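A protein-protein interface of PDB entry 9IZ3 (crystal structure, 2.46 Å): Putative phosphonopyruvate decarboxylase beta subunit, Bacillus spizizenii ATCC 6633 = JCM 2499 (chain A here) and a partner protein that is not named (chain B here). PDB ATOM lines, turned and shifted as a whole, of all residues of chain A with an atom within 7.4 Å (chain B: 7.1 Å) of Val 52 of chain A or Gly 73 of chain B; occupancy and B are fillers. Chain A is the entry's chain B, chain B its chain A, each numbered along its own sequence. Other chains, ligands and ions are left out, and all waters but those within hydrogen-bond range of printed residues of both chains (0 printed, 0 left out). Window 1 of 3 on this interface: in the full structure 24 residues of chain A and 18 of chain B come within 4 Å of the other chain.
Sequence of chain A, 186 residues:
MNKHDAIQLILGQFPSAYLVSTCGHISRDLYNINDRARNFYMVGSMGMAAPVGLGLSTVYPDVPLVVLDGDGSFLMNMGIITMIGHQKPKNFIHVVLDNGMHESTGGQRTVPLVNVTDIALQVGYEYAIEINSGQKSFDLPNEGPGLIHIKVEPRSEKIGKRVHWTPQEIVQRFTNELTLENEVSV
Along chain A the printed residues that touch a printed residue of chain B span positions 40 to 58.
Of the 20 printed residues of chain B, 8 touch a printed residue of chain A.
Printed residues of chain B that touch a printed residue of chain A: Asp 69, Ser 70, Gly 73, Val 74, Gly 77, Met 78, Leu 80 and Phe 104.
Hydrophobic or aromatic side chains of chain B that line the printed part of chain A: Val 74, Met 78, Leu 80 and Phe 104.
Gly 73 of chain B touches three residues of chain A.
Of the printed residues of chain B, Met 42 of chain A touches Phe 104 (3.6 Å).
Of the printed residues of chain B, Phe 40 of chain A touches Leu 80 (3.4 Å) and Phe 104 (3.8 Å).
Printed residues of chain B within 4 Å of Leu 56 of chain A: Gly 77 and Leu 80.
Ile 80 of chain A touches none of the printed residues of chain B.
Arg 67 of chain B touches none of the printed residues of chain A.
The nearest printed residue of chain A that does not touch Asp 69 of chain B is Pro 51 of chain A (5.0 Å).
O of Leu 54 of chain A sits at hydrogen-bond distance from OG1 of Thr 58 of chain A.
The side-chain carboxylate (OD1) of Asp 69 of chain B lies within salt-bridge range of the guanidinium group (NE) of Arg 67 of chain B, 3.4 Å away.
CD1 of Leu 80 of chain B touches CE2 of Phe 40 of chain A, at 3.4 Å.
SD of Met 42 of chain A touches CE1 of Phe 104 of chain B, at 3.6 Å.
SD of Met 48 of chain A touches CA of Gly 73 of chain B (3.9 Å).
Pro 51 of chain A touches Ser 70 of chain B (CB to O, 3.7 Å).
O of Gly 73 of chain B touches O of Pro 51 of chain A (3.5 Å).
Val 52 of chain A touches Gly 77 of chain B.
CD1 of Leu 80 of chain B touches CG1 of Val 52 of chain A, at 3.8 Å.
Leu 54 of chain A touches Val 74 of chain B (CD2 to CG2, 3.98 Å).
Gly 55 of chain A touches Val 74 of chain B (CA to O, 3.5 Å).
O of Gly 55 of chain A touches CG of Met 78 of chain B (3.7 Å).
The backbone carbonyl oxygen of Gly 73 of chain B lies close to the backbone NH of Val 52 of chain A, 3.4 Å away.
O of Asp 69 of chain B lies close to SD of Met 48 of chain A.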
ATOM      1  N   VAL A  20      -6.545  -1.986 -21.100  1.00  0.00           N
ATOM      2  CA  VAL A  20      -6.781  -0.589 -20.768  1.00  0.00           C
ATOM      3  C   VAL A  20      -5.434  -0.006 -20.362  1.00  0.00           C
ATOM      4  O   VAL A  20      -4.894  -0.354 -19.305  1.00  0.00           O
ATOM      5  CB  VAL A  20      -7.820  -0.432 -19.650  1.00  0.00           C
ATOM      6  CG1 VAL A  20      -8.167   1.032 -19.455  1.00  0.00           C
ATOM      7  CG2 VAL A  20      -9.066  -1.250 -19.968  1.00  0.00           C
ATOM      8  N   PHE A  40      -7.808  -0.398 -25.375  1.00  0.00           N
ATOM      9  CA  PHE A  40      -8.454   0.864 -25.032  1.00  0.00           C
ATOM     10  C   PHE A  40      -7.385   1.818 -24.505  1.00  0.00           C
ATOM     11  O   PHE A  40      -6.910   1.669 -23.373  1.00  0.00           O
ATOM     12  CB  PHE A  40      -9.569   0.657 -24.009  1.00  0.00           C
ATOM     13  CG  PHE A  40     -10.426   1.873 -23.799  1.00  0.00           C
ATOM     14  CD1 PHE A  40     -10.043   2.865 -22.907  1.00  0.00           C
ATOM     15  CD2 PHE A  40     -11.603   2.034 -24.508  1.00  0.00           C
ATOM     16  CE1 PHE A  40     -10.826   3.988 -22.721  1.00  0.00           C
ATOM     17  CE2 PHE A  40     -12.392   3.159 -24.331  1.00  0.00           C
ATOM     18  CZ  PHE A  40     -12.006   4.137 -23.435  1.00  0.00           C
ATOM     19  N   MET A  42      -5.851   5.423 -23.230  1.00  0.00           N
ATOM     20  CA  MET A  42      -6.220   6.630 -22.507  1.00  0.00           C
ATOM     21  C   MET A  42      -5.391   7.792 -23.034  1.00  0.00           C
ATOM     22  O   MET A  42      -4.163   7.694 -23.123  1.00  0.00           O
ATOM     23  CB  MET A  42      -6.003   6.458 -21.000  1.00  0.00           C
ATOM     24  CG  MET A  42      -6.824   5.337 -20.373  1.00  0.00           C
ATOM     25  SD  MET A  42      -8.548   5.790 -20.086  1.00  0.00           S
ATOM     26  CE  MET A  42      -8.336   7.011 -18.796  1.00  0.00           C
ATOM     27  N   GLY A  47      -4.662   7.934 -13.713  1.00  0.00           N
ATOM     28  CA  GLY A  47      -5.333   7.386 -12.552  1.00  0.00           C
ATOM     29  C   GLY A  47      -6.675   6.746 -12.835  1.00  0.00           C
ATOM     30  O   GLY A  47      -7.275   6.174 -11.915  1.00  0.00           O
ATOM     31  N   MET A  48      -7.160   6.811 -14.077  1.00  0.00           N
ATOM     32  CA  MET A  48      -8.471   6.290 -14.429  1.00  0.00           C
ATOM     33  C   MET A  48      -8.430   4.969 -15.187  1.00  0.00           C
ATOM     34  O   MET A  48      -9.491   4.370 -15.402  1.00  0.00           O
ATOM     35  CB  MET A  48      -9.243   7.326 -15.262  1.00  0.00           C
ATOM     36  CG  MET A  48      -9.733   8.514 -14.459  1.00  0.00           C
ATOM     37  SD  MET A  48     -10.846   8.012 -13.131  1.00  0.00           S
ATOM     38  CE  MET A  48      -9.824   8.298 -11.681  1.00  0.00           C
ATOM     39  N   ALA A  49      -7.249   4.497 -15.594  1.00  0.00           N
ATOM     40  CA  ALA A  49      -7.168   3.232 -16.314  1.00  0.00           C
ATOM     41  C   ALA A  49      -7.681   2.084 -15.460  1.00  0.00           C
ATOM     42  O   ALA A  49      -8.454   1.239 -15.934  1.00  0.00           O
ATOM     43  CB  ALA A  49      -5.730   2.964 -16.755  1.00  0.00           C
ATOM     44  N   ALA A  50      -7.282   2.049 -14.196  1.00  0.00           N
ATOM     45  CA  ALA A  50      -7.657   0.977 -13.285  1.00  0.00           C
ATOM     46  C   ALA A  50      -9.141   1.032 -12.922  1.00  0.00           C
ATOM     47  O   ALA A  50      -9.791  -0.019 -12.900  1.00  0.00           O
ATOM     48  CB  ALA A  50      -6.779   1.014 -12.029  1.00  0.00           C
ATOM     49  N   PRO A  51      -9.724   2.205 -12.620  1.00  0.00           N
ATOM     50  CA  PRO A  51     -11.191   2.242 -12.423  1.00  0.00           C
ATOM     51  C   PRO A  51     -11.984   1.794 -13.640  1.00  0.00           C
ATOM     52  O   PRO A  51     -12.957   1.035 -13.507  1.00  0.00           O
ATOM     53  CB  PRO A  51     -11.463   3.715 -12.085  1.00  0.00           C
ATOM     54  CG  PRO A  51     -10.188   4.235 -11.546  1.00  0.00           C
ATOM     55  CD  PRO A  51      -9.086   3.474 -12.221  1.00  0.00           C
ATOM     56  N   VAL A  52     -11.617   2.277 -14.827  1.00  0.00           N
ATOM     57  CA  VAL A  52     -12.322   1.873 -16.040  1.00  0.00           C
ATOM     58  C   VAL A  52     -12.208   0.370 -16.235  1.00  0.00           C
ATOM     59  O   VAL A  52     -13.196  -0.312 -16.550  1.00  0.00           O
ATOM     60  CB  VAL A  52     -11.778   2.657 -17.249  1.00  0.00           C
ATOM     61  CG1 VAL A  52     -12.252   2.043 -18.558  1.00  0.00           C
ATOM     62  CG2 VAL A  52     -12.198   4.112 -17.149  1.00  0.00           C
ATOM     63  N   GLY A  53     -11.009  -0.175 -16.019  1.00  0.00           N
ATOM     64  CA  GLY A  53     -10.832  -1.611 -16.130  1.00  0.00           C
ATOM     65  C   GLY A  53     -11.652  -2.379 -15.112  1.00  0.00           C
ATOM     66  O   GLY A  53     -12.178  -3.453 -15.408  1.00  0.00           O
ATOM     67  N   LEU A  54     -11.776  -1.836 -13.899  1.00  0.00           N
ATOM     68  CA  LEU A  54     -12.575  -2.498 -12.873  1.00  0.00           C
ATOM     69  C   LEU A  54     -14.047  -2.525 -13.259  1.00  0.00           C
ATOM     70  O   LEU A  54     -14.723  -3.547 -13.087  1.00  0.00           O
ATOM     71  CB  LEU A  54     -12.387  -1.798 -11.528  1.00  0.00           C
ATOM     72  CG  LEU A  54     -13.281  -2.322 -10.404  1.00  0.00           C
ATOM     73  CD1 LEU A  54     -12.999  -3.798 -10.158  1.00  0.00           C
ATOM     74  CD2 LEU A  54     -13.097  -1.508  -9.128  1.00  0.00           C
ATOM     75  N   GLY A  55     -14.564  -1.411 -13.774  1.00  0.00           N
ATOM     76  CA  GLY A  55     -15.932  -1.413 -14.272  1.00  0.00           C
ATOM     77  C   GLY A  55     -16.135  -2.442 -15.368  1.00  0.00           C
ATOM     78  O   GLY A  55     -17.110  -3.206 -15.359  1.00  0.00           O
ATOM     79  N   LEU A  56     -15.196  -2.491 -16.316  1.00  0.00           N
ATOM     80  CA  LEU A  56     -15.286  -3.445 -17.415  1.00  0.00           C
ATOM     81  C   LEU A  56     -15.307  -4.880 -16.900  1.00  0.00           C
ATOM     82  O   LEU A  56     -16.120  -5.698 -17.342  1.00  0.00           O
ATOM     83  CB  LEU A  56     -14.120  -3.236 -18.378  1.00  0.00           C
ATOM     84  CG  LEU A  56     -14.308  -2.137 -19.417  1.00  0.00           C
ATOM     85  CD1 LEU A  56     -12.954  -1.680 -19.923  1.00  0.00           C
ATOM     86  CD2 LEU A  56     -15.181  -2.644 -20.564  1.00  0.00           C
ATOM     87  N   SER A  57     -14.411  -5.203 -15.966  1.00  0.00           N
ATOM     88  CA  SER A  57     -14.380  -6.542 -15.392  1.00  0.00           C
ATOM     89  C   SER A  57     -15.609  -6.832 -14.542  1.00  0.00           C
ATOM     90  O   SER A  57     -15.923  -8.003 -14.306  1.00  0.00           O
ATOM     91  CB  SER A  57     -13.113  -6.728 -14.554  1.00  0.00           C
ATOM     92  OG  SER A  57     -11.966  -6.780 -15.383  1.00  0.00           O
ATOM     93  N   THR A  58     -16.291  -5.796 -14.054  1.00  0.00           N
ATOM     94  CA  THR A  58     -17.550  -6.010 -13.351  1.00  0.00           C
ATOM     95  C   THR A  58     -18.643  -6.429 -14.322  1.00  0.00           C
ATOM     96  O   THR A  58     -19.342  -7.425 -14.098  1.00  0.00           O
ATOM     97  CB  THR A  58     -17.965  -4.741 -12.608  1.00  0.00           C
ATOM     98  OG1 THR A  58     -17.006  -4.446 -11.586  1.00  0.00           O
ATOM     99  CG2 THR A  58     -19.332  -4.926 -11.977  1.00  0.00           C
ATOM    100  N   LEU A  65      -8.931  -9.179 -18.567  1.00  0.00           N
ATOM    101  CA  LEU A  65      -8.786  -7.735 -18.674  1.00  0.00           C
ATOM    102  C   LEU A  65      -7.469  -7.318 -18.046  1.00  0.00           C
ATOM    103  O   LEU A  65      -7.240  -7.563 -16.858  1.00  0.00           O
ATOM    104  CB  LEU A  65      -9.954  -7.015 -18.004  1.00  0.00           C
ATOM    105  CG  LEU A  65      -9.935  -5.534 -18.355  1.00  0.00           C
ATOM    106  CD1 LEU A  65     -11.234  -5.127 -18.999  1.00  0.00           C
ATOM    107  CD2 LEU A  65      -9.640  -4.713 -17.103  1.00  0.00           C
ATOM    108  N   VAL A  67      -5.007  -4.184 -17.133  1.00  0.00           N
ATOM    109  CA  VAL A  67      -4.773  -2.758 -16.937  1.00  0.00           C
ATOM    110  C   VAL A  67      -3.268  -2.531 -16.927  1.00  0.00           C
ATOM    111  O   VAL A  67      -2.531  -3.240 -16.229  1.00  0.00           O
ATOM    112  CB  VAL A  67      -5.409  -2.262 -15.628  1.00  0.00           C
ATOM    113  CG1 VAL A  67      -4.923  -0.851 -15.306  1.00  0.00           C
ATOM    114  CG2 VAL A  67      -6.926  -2.315 -15.716  1.00  0.00           C
ATOM    115  N   ILE A  80      -7.693   2.788  -5.497  1.00  0.00           N
ATOM    116  CA  ILE A  80      -8.444   1.894  -6.376  1.00  0.00           C
ATOM    117  C   ILE A  80      -8.234   0.441  -5.982  1.00  0.00           C
ATOM    118  O   ILE A  80      -9.166  -0.373  -6.059  1.00  0.00           O
ATOM    119  CB  ILE A  80      -8.067   2.135  -7.857  1.00  0.00           C
ATOM    120  CG1 ILE A  80      -8.922   1.267  -8.770  1.00  0.00           C
ATOM    121  CG2 ILE A  80      -6.618   1.764  -8.116  1.00  0.00           C
ATOM    122  CD1 ILE A  80     -10.282   1.805  -9.010  1.00  0.00           C
ATOM    123  N   PHE A  92      -8.918 -10.263 -13.880  1.00  0.00           N
ATOM    124  CA  PHE A  92      -8.355  -8.922 -13.840  1.00  0.00           C
ATOM    125  C   PHE A  92      -6.860  -9.030 -13.564  1.00  0.00           C
ATOM    126  O   PHE A  92      -6.447  -9.699 -12.611  1.00  0.00           O
ATOM    127  CB  PHE A  92      -9.057  -8.101 -12.756  1.00  0.00           C
ATOM    128  CG  PHE A  92      -8.666  -6.657 -12.724  1.00  0.00           C
ATOM    129  CD1 PHE A  92      -7.613  -6.227 -11.935  1.00  0.00           C
ATOM    130  CD2 PHE A  92      -9.374  -5.720 -13.455  1.00  0.00           C
ATOM    131  CE1 PHE A  92      -7.263  -4.893 -11.892  1.00  0.00           C
ATOM    132  CE2 PHE A  92      -9.028  -4.385 -13.419  1.00  0.00           C
ATOM    133  CZ  PHE A  92      -7.975  -3.969 -12.637  1.00  0.00           C
ATOM    134  N   PHE A 174     -13.405  -0.746 -29.698  1.00  0.00           N
ATOM    135  CA  PHE A 174     -13.234  -1.542 -28.487  1.00  0.00           C
ATOM    136  C   PHE A 174     -14.552  -2.168 -28.043  1.00  0.00           C
ATOM    137  O   PHE A 174     -14.627  -3.380 -27.783  1.00  0.00           O
ATOM    138  CB  PHE A 174     -12.643  -0.657 -27.383  1.00  0.00           C
ATOM    139  CG  PHE A 174     -12.353  -1.382 -26.101  1.00  0.00           C
ATOM    140  CD1 PHE A 174     -11.166  -2.076 -25.933  1.00  0.00           C
ATOM    141  CD2 PHE A 174     -13.261  -1.355 -25.056  1.00  0.00           C
ATOM    142  CE1 PHE A 174     -10.894  -2.742 -24.749  1.00  0.00           C
ATOM    143  CE2 PHE A 174     -12.997  -2.017 -23.867  1.00  0.00           C
ATOM    144  CZ  PHE A 174     -11.810  -2.711 -23.713  1.00  0.00           C
ATOM    145  N   THR B  35     -22.804   3.677  -9.226  1.00  0.00           N
ATOM    146  CA  THR B  35     -21.622   3.854  -8.394  1.00  0.00           C
ATOM    147  C   THR B  35     -21.778   5.094  -7.524  1.00  0.00           C
ATOM    148  O   THR B  35     -22.652   5.931  -7.755  1.00  0.00           O
ATOM    149  CB  THR B  35     -20.336   3.973  -9.226  1.00  0.00           C
ATOM    150  OG1 THR B  35     -20.302   5.248  -9.876  1.00  0.00           O
ATOM    151  CG2 THR B  35     -20.254   2.870 -10.270  1.00  0.00           C
ATOM    152  N   ARG B  67     -13.666   7.232  -3.681  1.00  0.00           N
ATOM    153  CA  ARG B  67     -13.673   8.638  -4.058  1.00  0.00           C
ATOM    154  C   ARG B  67     -14.436   8.800  -5.364  1.00  0.00           C
ATOM    155  O   ARG B  67     -14.631   7.841  -6.115  1.00  0.00           O
ATOM    156  CB  ARG B  67     -12.251   9.196  -4.189  1.00  0.00           C
ATOM    157  CG  ARG B  67     -12.171  10.698  -3.983  1.00  0.00           C
ATOM    158  CD  ARG B  67     -10.750  11.161  -3.746  1.00  0.00           C
ATOM    159  NE  ARG B  67     -10.140  11.694  -4.958  1.00  0.00           N
ATOM    160  CZ  ARG B  67      -9.242  12.674  -4.967  1.00  0.00           C
ATOM    161  NH1 ARG B  67      -8.854  13.227  -3.825  1.00  0.00           N
ATOM    162  NH2 ARG B  67      -8.732  13.100  -6.115  1.00  0.00           N
ATOM    163  N   GLU B  68     -14.850  10.040  -5.634  1.00  0.00           N
ATOM    164  CA  GLU B  68     -15.763  10.299  -6.744  1.00  0.00           C
ATOM    165  C   GLU B  68     -15.109  10.029  -8.093  1.00  0.00           C
ATOM    166  O   GLU B  68     -15.763   9.516  -9.008  1.00  0.00           O
ATOM    167  CB  GLU B  68     -16.277  11.735  -6.678  1.00  0.00           C
ATOM    168  CG  GLU B  68     -17.299  11.981  -5.583  1.00  0.00           C
ATOM    169  CD  GLU B  68     -16.654  12.410  -4.278  1.00  0.00           C
ATOM    170  OE1 GLU B  68     -15.458  12.768  -4.294  1.00  0.00           O
ATOM    171  OE2 GLU B  68     -17.345  12.390  -3.237  1.00  0.00           O
ATOM    172  N   ASP B  69     -13.828  10.380  -8.249  1.00  0.00           N
ATOM    173  CA  ASP B  69     -13.154  10.136  -9.522  1.00  0.00           C
ATOM    174  C   ASP B  69     -13.076   8.642  -9.826  1.00  0.00           C
ATOM    175  O   ASP B  69     -13.242   8.220 -10.978  1.00  0.00           O
ATOM    176  CB  ASP B  69     -11.759  10.768  -9.516  1.00  0.00           C
ATOM    177  CG  ASP B  69     -10.849  10.177  -8.455  1.00  0.00           C
ATOM    178  OD1 ASP B  69     -11.362   9.687  -7.429  1.00  0.00           O
ATOM    179  OD2 ASP B  69      -9.615  10.199  -8.652  1.00  0.00           O
ATOM    180  N   SER B  70     -12.853   7.822  -8.797  1.00  0.00           N
ATOM    181  CA  SER B  70     -12.864   6.379  -9.007  1.00  0.00           C
ATOM    182  C   SER B  70     -14.261   5.882  -9.358  1.00  0.00           C
ATOM    183  O   SER B  70     -14.414   4.972 -10.182  1.00  0.00           O
ATOM    184  CB  SER B  70     -12.330   5.668  -7.769  1.00  0.00           C
ATOM    185  OG  SER B  70     -10.917   5.607  -7.804  1.00  0.00           O
ATOM    186  N   ALA B  71     -15.292   6.460  -8.738  1.00  0.00           N
ATOM    187  CA  ALA B  71     -16.660   6.101  -9.093  1.00  0.00           C
ATOM    188  C   ALA B  71     -16.943   6.428 -10.553  1.00  0.00           C
ATOM    189  O   ALA B  71     -17.569   5.636 -11.266  1.00  0.00           O
ATOM    190  CB  ALA B  71     -17.644   6.823  -8.176  1.00  0.00           C
ATOM    191  N   LEU B  72     -16.464   7.582 -11.017  1.00  0.00           N
ATOM    192  CA  LEU B  72     -16.633   7.962 -12.414  1.00  0.00           C
ATOM    193  C   LEU B  72     -15.902   7.002 -13.343  1.00  0.00           C
ATOM    194  O   LEU B  72     -16.443   6.604 -14.380  1.00  0.00           O
ATOM    195  CB  LEU B  72     -16.149   9.397 -12.621  1.00  0.00           C
ATOM    196  CG  LEU B  72     -16.399  10.022 -13.993  1.00  0.00           C
ATOM    197  CD1 LEU B  72     -17.796   9.686 -14.507  1.00  0.00           C
ATOM    198  CD2 LEU B  72     -16.192  11.519 -13.930  1.00  0.00           C
ATOM    199  N   GLY B  73     -14.670   6.627 -12.995  1.00  0.00           N
ATOM    200  CA  GLY B  73     -13.944   5.675 -13.821  1.00  0.00           C
ATOM    201  C   GLY B  73     -14.632   4.325 -13.897  1.00  0.00           C
ATOM    202  O   GLY B  73     -14.728   3.724 -14.972  1.00  0.00           O
ATOM    203  N   VAL B  74     -15.127   3.833 -12.757  1.00  0.00           N
ATOM    204  CA  VAL B  74     -15.832   2.554 -12.738  1.00  0.00           C
ATOM    205  C   VAL B  74     -17.100   2.635 -13.580  1.00  0.00           C
ATOM    206  O   VAL B  74     -17.417   1.713 -14.343  1.00  0.00           O
ATOM    207  CB  VAL B  74     -16.139   2.132 -11.287  1.00  0.00           C
ATOM    208  CG1 VAL B  74     -17.123   0.971 -11.259  1.00  0.00           C
ATOM    209  CG2 VAL B  74     -14.861   1.752 -10.570  1.00  0.00           C
ATOM    210  N   ALA B  75     -17.839   3.741 -13.460  1.00  0.00           N
ATOM    211  CA  ALA B  75     -19.051   3.914 -14.253  1.00  0.00           C
ATOM    212  C   ALA B  75     -18.734   3.950 -15.742  1.00  0.00           C
ATOM    213  O   ALA B  75     -19.434   3.326 -16.549  1.00  0.00           O
ATOM    214  CB  ALA B  75     -19.777   5.188 -13.822  1.00  0.00           C
ATOM    215  N   SER B  76     -17.676   4.670 -16.125  1.00  0.00           N
ATOM    216  CA  SER B  76     -17.276   4.726 -17.527  1.00  0.00           C
ATOM    217  C   SER B  76     -16.892   3.348 -18.054  1.00  0.00           C
ATOM    218  O   SER B  76     -17.253   2.980 -19.180  1.00  0.00           O
ATOM    219  CB  SER B  76     -16.122   5.710 -17.689  1.00  0.00           C
ATOM    220  OG  SER B  76     -16.482   6.989 -17.195  1.00  0.00           O
ATOM    221  N   GLY B  77     -16.162   2.569 -17.255  1.00  0.00           N
ATOM    222  CA  GLY B  77     -15.837   1.213 -17.672  1.00  0.00           C
ATOM    223  C   GLY B  77     -17.073   0.349 -17.842  1.00  0.00           C
ATOM    224  O   GLY B  77     -17.180  -0.427 -18.797  1.00  0.00           O
ATOM    225  N   MET B  78     -18.023   0.473 -16.912  1.00  0.00           N
ATOM    226  CA  MET B  78     -19.282  -0.250 -17.037  1.00  0.00           C
ATOM    227  C   MET B  78     -19.997   0.123 -18.326  1.00  0.00           C
ATOM    228  O   MET B  78     -20.509  -0.748 -19.038  1.00  0.00           O
ATOM    229  CB  MET B  78     -20.172   0.039 -15.830  1.00  0.00           C
ATOM    230  CG  MET B  78     -19.854  -0.800 -14.604  1.00  0.00           C
ATOM    231  SD  MET B  78     -20.748  -0.223 -13.148  1.00  0.00           S
ATOM    232  CE  MET B  78     -20.990  -1.772 -12.286  1.00  0.00           C
ATOM    233  N   TYR B  79     -20.031   1.419 -18.643  1.00  0.00           N
ATOM    234  CA  TYR B  79     -20.632   1.858 -19.897  1.00  0.00           C
ATOM    235  C   TYR B  79     -19.937   1.218 -21.089  1.00  0.00           C
ATOM    236  O   TYR B  79     -20.595   0.790 -22.045  1.00  0.00           O
ATOM    237  CB  TYR B  79     -20.585   3.379 -20.014  1.00  0.00           C
ATOM    238  CG  TYR B  79     -21.134   3.867 -21.333  1.00  0.00           C
ATOM    239  CD1 TYR B  79     -22.496   4.071 -21.505  1.00  0.00           C
ATOM    240  CD2 TYR B  79     -20.295   4.097 -22.418  1.00  0.00           C
ATOM    241  CE1 TYR B  79     -23.005   4.504 -22.710  1.00  0.00           C
ATOM    242  CE2 TYR B  79     -20.796   4.530 -23.626  1.00  0.00           C
ATOM    243  CZ  TYR B  79     -22.151   4.731 -23.768  1.00  0.00           C
ATOM    244  OH  TYR B  79     -22.657   5.166 -24.972  1.00  0.00           O
ATOM    245  N   LEU B  80     -18.605   1.163 -21.058  1.00  0.00           N
ATOM    246  CA  LEU B  80     -17.877   0.488 -22.128  1.00  0.00           C
ATOM    247  C   LEU B  80     -18.250  -0.985 -22.206  1.00  0.00           C
ATOM    248  O   LEU B  80     -18.202  -1.586 -23.287  1.00  0.00           O
ATOM    249  CB  LEU B  80     -16.374   0.642 -21.921  1.00  0.00           C
ATOM    250  CG  LEU B  80     -15.858   2.074 -22.011  1.00  0.00           C
ATOM    251  CD1 LEU B  80     -14.367   2.093 -21.763  1.00  0.00           C
ATOM    252  CD2 LEU B  80     -16.199   2.685 -23.361  1.00  0.00           C
ATOM    253  N   MET B  87     -24.004   7.658 -11.437  1.00  0.00           N
ATOM    254  CA  MET B  87     -23.184   7.828 -10.250  1.00  0.00           C
ATOM    255  C   MET B  87     -23.804   8.862  -9.321  1.00  0.00           C
ATOM    256  O   MET B  87     -24.120   9.979  -9.742  1.00  0.00           O
ATOM    257  CB  MET B  87     -21.761   8.233 -10.624  1.00  0.00           C
ATOM    258  CG  MET B  87     -20.826   8.332  -9.437  1.00  0.00           C
ATOM    259  SD  MET B  87     -19.591   9.618  -9.692  1.00  0.00           S
ATOM    260  CE  MET B  87     -19.226   9.385 -11.425  1.00  0.00           C
ATOM    261  N   VAL B 100     -11.522  14.512 -15.155  1.00  0.00           N
ATOM    262  CA  VAL B 100     -12.033  13.298 -15.791  1.00  0.00           C
ATOM    263  C   VAL B 100     -13.123  13.660 -16.793  1.00  0.00           C
ATOM    264  O   VAL B 100     -12.981  13.440 -18.003  1.00  0.00           O
ATOM    265  CB  VAL B 100     -12.543  12.304 -14.732  1.00  0.00           C
ATOM    266  CG1 VAL B 100     -12.843  10.947 -15.367  1.00  0.00           C
ATOM    267  CG2 VAL B 100     -11.523  12.151 -13.612  1.00  0.00           C
ATOM    268  N   PHE B 104     -11.956  12.988 -20.375  1.00  0.00           N
ATOM    269  CA  PHE B 104     -12.270  11.603 -20.714  1.00  0.00           C
ATOM    270  C   PHE B 104     -13.674  11.482 -21.293  1.00  0.00           C
ATOM    271  O   PHE B 104     -13.813  11.237 -22.495  1.00  0.00           O
ATOM    272  CB  PHE B 104     -12.087  10.721 -19.477  1.00  0.00           C
ATOM    273  CG  PHE B 104     -12.320   9.267 -19.733  1.00  0.00           C
ATOM    274  CD1 PHE B 104     -11.527   8.579 -20.634  1.00  0.00           C
ATOM    275  CD2 PHE B 104     -13.336   8.587 -19.081  1.00  0.00           C
ATOM    276  CE1 PHE B 104     -11.736   7.236 -20.877  1.00  0.00           C
ATOM    277  CE2 PHE B 104     -13.549   7.244 -19.318  1.00  0.00           C
ATOM    278  CZ  PHE B 104     -12.747   6.566 -20.218  1.00  0.00           C
ATOM    279  N   ASN B 105     -14.729  11.649 -20.486  1.00  0.00           N
ATOM    280  CA  ASN B 105     -16.081  11.381 -20.972  1.00  0.00           C
ATOM    281  C   ASN B 105     -16.558  12.397 -21.996  1.00  0.00           C
ATOM    282  O   ASN B 105     -17.397  12.058 -22.838  1.00  0.00           O
ATOM    283  CB  ASN B 105     -17.073  11.327 -19.810  1.00  0.00           C
ATOM    284  CG  ASN B 105     -16.568  10.490 -18.655  1.00  0.00           C
ATOM    285  OD1 ASN B 105     -15.829  10.982 -17.805  1.00  0.00           O
ATOM    286  ND2 ASN B 105     -16.966   9.221 -18.613  1.00  0.00           N
ATOM    287  N   ILE B 110     -18.559   9.329 -23.430  1.00  0.00           N
ATOM    288  CA  ILE B 110     -19.059   8.263 -22.566  1.00  0.00           C
ATOM    289  C   ILE B 110     -20.103   8.865 -21.633  1.00  0.00           C
ATOM    290  O   ILE B 110     -19.747   9.507 -20.635  1.00  0.00           O
ATOM    291  CB  ILE B 110     -17.919   7.587 -21.791  1.00  0.00           C
ATOM    292  CG1 ILE B 110     -16.974   6.879 -22.760  1.00  0.00           C
ATOM    293  CG2 ILE B 110     -18.470   6.588 -20.782  1.00  0.00           C
ATOM    294  CD1 ILE B 110     -15.689   6.423 -22.116  1.00  0.00           C
